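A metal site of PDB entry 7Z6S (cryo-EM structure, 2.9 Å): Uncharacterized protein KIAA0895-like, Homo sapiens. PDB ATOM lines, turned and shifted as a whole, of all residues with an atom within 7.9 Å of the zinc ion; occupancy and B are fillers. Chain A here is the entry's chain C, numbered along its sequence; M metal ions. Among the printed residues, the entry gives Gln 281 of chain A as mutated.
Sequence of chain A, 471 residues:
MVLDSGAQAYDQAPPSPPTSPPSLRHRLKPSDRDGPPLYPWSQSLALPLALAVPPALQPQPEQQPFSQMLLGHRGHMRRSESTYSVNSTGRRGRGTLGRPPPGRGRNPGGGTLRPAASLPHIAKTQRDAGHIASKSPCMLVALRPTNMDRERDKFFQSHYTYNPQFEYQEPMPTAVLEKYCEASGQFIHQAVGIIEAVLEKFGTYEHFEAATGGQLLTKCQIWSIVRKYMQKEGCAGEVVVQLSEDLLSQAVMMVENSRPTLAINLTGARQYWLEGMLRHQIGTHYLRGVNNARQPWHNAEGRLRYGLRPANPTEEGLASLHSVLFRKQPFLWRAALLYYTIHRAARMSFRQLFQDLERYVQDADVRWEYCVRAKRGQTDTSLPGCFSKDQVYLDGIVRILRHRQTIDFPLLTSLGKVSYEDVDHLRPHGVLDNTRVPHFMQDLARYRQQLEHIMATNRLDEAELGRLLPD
ND1 of His 280 lies within hydrogen-bond range of O of Ala 319, at 3.1 Å. ND1 of His 280 is in hydrogen-bond range of OG of Ser 323 (3.0 Å). O of Glu 316 lies within hydrogen-bond range of OG of Ser 320 (2.9 Å). The backbone NH (N) of Glu 316 is in hydrogen-bond range of the side-chain amide oxygen (OD1) of Asn 312. The side-chain carboxylate of Glu 315 is in hydrogen-bond range of a ring nitrogen (ND1) of His 285.
OH of Tyr 393 touches the zinc ion, at 3.9 Å. Four residues have an atom within 4 Å of the zinc ion: His 280, His 285, Glu 316 and Tyr 393.
NE2 of His 280 is bound to the zinc ion (2.2 Å). The zinc ion is bound by the side-chain carboxylate (OE1) of Glu 316 (2.3 Å). The zinc ion is bound by NE2 of His 285 (2.5 Å). Slightly farther from the zinc ion lies OE2 of Glu 316 (2.8 Å).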
ATOM      1  N   SER A 249     -25.357 -23.140 -14.132  1.00  0.00           N
ATOM      2  CA  SER A 249     -24.272 -22.620 -13.301  1.00  0.00           C
ATOM      3  C   SER A 249     -23.818 -23.676 -12.291  1.00  0.00           C
ATOM      4  O   SER A 249     -24.348 -24.780 -12.246  1.00  0.00           O
ATOM      5  CB  SER A 249     -24.721 -21.343 -12.574  1.00  0.00           C
ATOM      6  OG  SER A 249     -25.815 -21.592 -11.733  1.00  0.00           O
ATOM      7  N   ALA A 251     -24.069 -23.455  -8.985  1.00  0.00           N
ATOM      8  CA  ALA A 251     -25.135 -23.582  -7.997  1.00  0.00           C
ATOM      9  C   ALA A 251     -26.159 -22.453  -8.108  1.00  0.00           C
ATOM     10  O   ALA A 251     -25.830 -21.365  -8.567  1.00  0.00           O
ATOM     11  CB  ALA A 251     -24.532 -23.634  -6.594  1.00  0.00           C
ATOM     12  N   VAL A 252     -27.390 -22.711  -7.674  1.00  0.00           N
ATOM     13  CA  VAL A 252     -28.448 -21.714  -7.579  1.00  0.00           C
ATOM     14  C   VAL A 252     -29.168 -21.808  -6.235  1.00  0.00           C
ATOM     15  O   VAL A 252     -29.598 -22.870  -5.816  1.00  0.00           O
ATOM     16  CB  VAL A 252     -29.465 -21.839  -8.747  1.00  0.00           C
ATOM     17  CG1 VAL A 252     -30.133 -23.207  -8.749  1.00  0.00           C
ATOM     18  CG2 VAL A 252     -30.504 -20.724  -8.675  1.00  0.00           C
ATOM     19  N   MET A 253     -29.244 -20.675  -5.536  1.00  0.00           N
ATOM     20  CA  MET A 253     -29.992 -20.546  -4.285  1.00  0.00           C
ATOM     21  C   MET A 253     -31.431 -20.237  -4.658  1.00  0.00           C
ATOM     22  O   MET A 253     -31.664 -19.362  -5.456  1.00  0.00           O
ATOM     23  CB  MET A 253     -29.373 -19.444  -3.428  1.00  0.00           C
ATOM     24  CG  MET A 253     -29.913 -19.409  -2.013  1.00  0.00           C
ATOM     25  SD  MET A 253     -29.228 -20.769  -1.040  1.00  0.00           S
ATOM     26  CE  MET A 253     -30.229 -20.647   0.433  1.00  0.00           C
ATOM     27  N   MET A 277     -18.057 -21.274  -4.000  1.00  0.00           N
ATOM     28  CA  MET A 277     -19.493 -21.300  -4.327  1.00  0.00           C
ATOM     29  C   MET A 277     -20.346 -21.076  -3.072  1.00  0.00           C
ATOM     30  O   MET A 277     -21.320 -20.319  -3.096  1.00  0.00           O
ATOM     31  CB  MET A 277     -19.874 -22.631  -4.988  1.00  0.00           C
ATOM     32  CG  MET A 277     -21.371 -22.787  -5.320  1.00  0.00           C
ATOM     33  SD  MET A 277     -22.419 -23.210  -3.909  1.00  0.00           S
ATOM     34  CE  MET A 277     -21.831 -24.874  -3.544  1.00  0.00           C
ATOM     35  N   HIS A 280     -20.255 -17.590  -1.933  1.00  0.00           N
ATOM     36  CA  HIS A 280     -21.098 -16.844  -2.856  1.00  0.00           C
ATOM     37  C   HIS A 280     -22.580 -17.014  -2.482  1.00  0.00           C
ATOM     38  O   HIS A 280     -23.257 -16.044  -2.127  1.00  0.00           O
ATOM     39  CB  HIS A 280     -20.837 -17.337  -4.292  1.00  0.00           C
ATOM     40  CG  HIS A 280     -21.643 -16.632  -5.343  1.00  0.00           C
ATOM     41  ND1 HIS A 280     -21.066 -15.905  -6.367  1.00  0.00           N
ATOM     42  CD2 HIS A 280     -22.975 -16.569  -5.563  1.00  0.00           C
ATOM     43  CE1 HIS A 280     -22.001 -15.417  -7.148  1.00  0.00           C
ATOM     44  NE2 HIS A 280     -23.178 -15.791  -6.674  1.00  0.00           N
ATOM     45  N   GLN A 281     -23.103 -18.242  -2.605  1.00  0.00           N
ATOM     46  CA  GLN A 281     -24.535 -18.452  -2.370  1.00  0.00           C
ATOM     47  C   GLN A 281     -24.979 -18.306  -0.920  1.00  0.00           C
ATOM     48  O   GLN A 281     -25.995 -17.687  -0.636  1.00  0.00           O
ATOM     49  CB  GLN A 281     -24.950 -19.826  -2.885  1.00  0.00           C
ATOM     50  CG  GLN A 281     -24.216 -20.249  -4.145  1.00  0.00           C
ATOM     51  CD  GLN A 281     -25.129 -20.328  -5.351  1.00  0.00           C
ATOM     52  OE1 GLN A 281     -24.809 -19.809  -6.413  1.00  0.00           O
ATOM     53  NE2 GLN A 281     -26.278 -20.966  -5.181  1.00  0.00           N
ATOM     54  N   THR A 284     -23.038 -14.885   1.044  1.00  0.00           N
ATOM     55  CA  THR A 284     -23.522 -13.615   0.505  1.00  0.00           C
ATOM     56  C   THR A 284     -25.048 -13.629   0.280  1.00  0.00           C
ATOM     57  O   THR A 284     -25.777 -13.006   1.047  1.00  0.00           O
ATOM     58  CB  THR A 284     -22.763 -13.224  -0.781  1.00  0.00           C
ATOM     59  OG1 THR A 284     -21.364 -13.495  -0.602  1.00  0.00           O
ATOM     60  CG2 THR A 284     -22.942 -11.757  -1.120  1.00  0.00           C
ATOM     61  N   HIS A 285     -25.519 -14.354  -0.743  1.00  0.00           N
ATOM     62  CA  HIS A 285     -26.945 -14.332  -1.116  1.00  0.00           C
ATOM     63  C   HIS A 285     -27.878 -14.685   0.032  1.00  0.00           C
ATOM     64  O   HIS A 285     -28.836 -13.963   0.293  1.00  0.00           O
ATOM     65  CB  HIS A 285     -27.232 -15.240  -2.318  1.00  0.00           C
ATOM     66  CG  HIS A 285     -26.603 -14.772  -3.587  1.00  0.00           C
ATOM     67  ND1 HIS A 285     -26.465 -13.443  -3.913  1.00  0.00           N
ATOM     68  CD2 HIS A 285     -26.084 -15.472  -4.629  1.00  0.00           C
ATOM     69  CE1 HIS A 285     -25.853 -13.338  -5.084  1.00  0.00           C
ATOM     70  NE2 HIS A 285     -25.616 -14.559  -5.537  1.00  0.00           N
ATOM     71  N   ASN A 312     -28.768  -5.417  -7.340  1.00  0.00           N
ATOM     72  CA  ASN A 312     -27.718  -5.603  -8.315  1.00  0.00           C
ATOM     73  C   ASN A 312     -27.304  -4.249  -8.895  1.00  0.00           C
ATOM     74  O   ASN A 312     -28.137  -3.357  -9.009  1.00  0.00           O
ATOM     75  CB  ASN A 312     -28.174  -6.544  -9.427  1.00  0.00           C
ATOM     76  CG  ASN A 312     -27.952  -8.002  -9.080  1.00  0.00           C
ATOM     77  OD1 ASN A 312     -26.995  -8.334  -8.386  1.00  0.00           O
ATOM     78  ND2 ASN A 312     -28.810  -8.884  -9.580  1.00  0.00           N
ATOM     79  N   GLU A 315     -25.126  -6.938  -5.341  1.00  0.00           N
ATOM     80  CA  GLU A 315     -25.373  -8.280  -4.838  1.00  0.00           C
ATOM     81  C   GLU A 315     -24.408  -9.316  -5.429  1.00  0.00           C
ATOM     82  O   GLU A 315     -23.670  -9.995  -4.710  1.00  0.00           O
ATOM     83  CB  GLU A 315     -26.832  -8.683  -5.105  1.00  0.00           C
ATOM     84  CG  GLU A 315     -27.270 -10.018  -4.506  1.00  0.00           C
ATOM     85  CD  GLU A 315     -27.315 -10.009  -2.986  1.00  0.00           C
ATOM     86  OE1 GLU A 315     -27.397  -8.908  -2.384  1.00  0.00           O
ATOM     87  OE2 GLU A 315     -27.287 -11.113  -2.398  1.00  0.00           O
ATOM     88  N   GLU A 316     -24.437  -9.445  -6.762  1.00  0.00           N
ATOM     89  CA  GLU A 316     -23.646 -10.441  -7.471  1.00  0.00           C
ATOM     90  C   GLU A 316     -22.183 -10.052  -7.575  1.00  0.00           C
ATOM     91  O   GLU A 316     -21.331 -10.911  -7.748  1.00  0.00           O
ATOM     92  CB  GLU A 316     -24.231 -10.687  -8.843  1.00  0.00           C
ATOM     93  CG  GLU A 316     -25.625 -11.302  -8.828  1.00  0.00           C
ATOM     94  CD  GLU A 316     -25.659 -12.761  -8.401  1.00  0.00           C
ATOM     95  OE1 GLU A 316     -24.672 -13.271  -7.810  1.00  0.00           O
ATOM     96  OE2 GLU A 316     -26.701 -13.404  -8.658  1.00  0.00           O
ATOM     97  N   GLY A 317     -21.886  -8.749  -7.462  1.00  0.00           N
ATOM     98  CA  GLY A 317     -20.530  -8.239  -7.364  1.00  0.00           C
ATOM     99  C   GLY A 317     -19.857  -8.717  -6.090  1.00  0.00           C
ATOM    100  O   GLY A 317     -18.741  -9.225  -6.118  1.00  0.00           O
ATOM    101  N   ALA A 319     -20.915 -11.209  -4.170  1.00  0.00           N
ATOM    102  CA  ALA A 319     -20.932 -12.664  -4.197  1.00  0.00           C
ATOM    103  C   ALA A 319     -19.761 -13.238  -5.014  1.00  0.00           C
ATOM    104  O   ALA A 319     -19.171 -14.248  -4.628  1.00  0.00           O
ATOM    105  CB  ALA A 319     -22.266 -13.164  -4.750  1.00  0.00           C
ATOM    106  N   SER A 320     -19.443 -12.581  -6.142  1.00  0.00           N
ATOM    107  CA  SER A 320     -18.352 -12.989  -7.024  1.00  0.00           C
ATOM    108  C   SER A 320     -16.975 -12.765  -6.413  1.00  0.00           C
ATOM    109  O   SER A 320     -16.082 -13.600  -6.569  1.00  0.00           O
ATOM    110  CB  SER A 320     -18.441 -12.269  -8.374  1.00  0.00           C
ATOM    111  OG  SER A 320     -19.562 -12.729  -9.110  1.00  0.00           O
ATOM    112  N   SER A 323     -16.452 -15.465  -3.824  1.00  0.00           N
ATOM    113  CA  SER A 323     -16.204 -16.800  -4.357  1.00  0.00           C
ATOM    114  C   SER A 323     -14.699 -17.071  -4.474  1.00  0.00           C
ATOM    115  O   SER A 323     -14.225 -18.189  -4.212  1.00  0.00           O
ATOM    116  CB  SER A 323     -16.856 -17.038  -5.727  1.00  0.00           C
ATOM    117  OG  SER A 323     -18.199 -16.608  -5.874  1.00  0.00           O
ATOM    118  N   ARG A 373     -26.552 -19.248 -21.813  1.00  0.00           N
ATOM    119  CA  ARG A 373     -26.669 -18.215 -20.791  1.00  0.00           C
ATOM    120  C   ARG A 373     -26.763 -16.813 -21.377  1.00  0.00           C
ATOM    121  O   ARG A 373     -27.550 -15.985 -20.913  1.00  0.00           O
ATOM    122  CB  ARG A 373     -25.506 -18.296 -19.808  1.00  0.00           C
ATOM    123  CG  ARG A 373     -25.616 -19.423 -18.800  1.00  0.00           C
ATOM    124  CD  ARG A 373     -24.488 -19.284 -17.799  1.00  0.00           C
ATOM    125  NE  ARG A 373     -24.613 -18.194 -16.843  1.00  0.00           N
ATOM    126  CZ  ARG A 373     -25.310 -18.246 -15.705  1.00  0.00           C
ATOM    127  NH1 ARG A 373     -26.042 -19.315 -15.405  1.00  0.00           N
ATOM    128  NH2 ARG A 373     -25.343 -17.188 -14.900  1.00  0.00           N
ATOM    129  N   VAL A 392     -23.707  -8.519 -14.895  1.00  0.00           N
ATOM    130  CA  VAL A 392     -23.804  -7.965 -13.552  1.00  0.00           C
ATOM    131  C   VAL A 392     -22.596  -8.308 -12.674  1.00  0.00           C
ATOM    132  O   VAL A 392     -22.185  -7.485 -11.860  1.00  0.00           O
ATOM    133  CB  VAL A 392     -25.108  -8.448 -12.890  1.00  0.00           C
ATOM    134  CG1 VAL A 392     -25.063  -9.941 -12.604  1.00  0.00           C
ATOM    135  CG2 VAL A 392     -25.370  -7.643 -11.667  1.00  0.00           C
ATOM    136  N   TYR A 393     -22.031  -9.510 -12.870  1.00  0.00           N
ATOM    137  CA  TYR A 393     -20.938 -10.012 -12.042  1.00  0.00           C
ATOM    138  C   TYR A 393     -19.708  -9.102 -12.122  1.00  0.00           C
ATOM    139  O   TYR A 393     -19.257  -8.571 -11.108  1.00  0.00           O
ATOM    140  CB  TYR A 393     -20.591 -11.442 -12.418  1.00  0.00           C
ATOM    141  CG  TYR A 393     -21.723 -12.415 -12.234  1.00  0.00           C
ATOM    142  CD1 TYR A 393     -22.125 -12.795 -10.982  1.00  0.00           C
ATOM    143  CD2 TYR A 393     -22.393 -12.955 -13.320  1.00  0.00           C
ATOM    144  CE1 TYR A 393     -23.171 -13.692 -10.789  1.00  0.00           C
ATOM    145  CE2 TYR A 393     -23.443 -13.841 -13.158  1.00  0.00           C
ATOM    146  CZ  TYR A 393     -23.808 -14.218 -11.877  1.00  0.00           C
ATOM    147  OH  TYR A 393     -24.841 -15.113 -11.695  1.00  0.00           O
HETATM  148 ZN    ZN M   1     -25.086 -15.520  -7.790  1.00  0.00          ZN
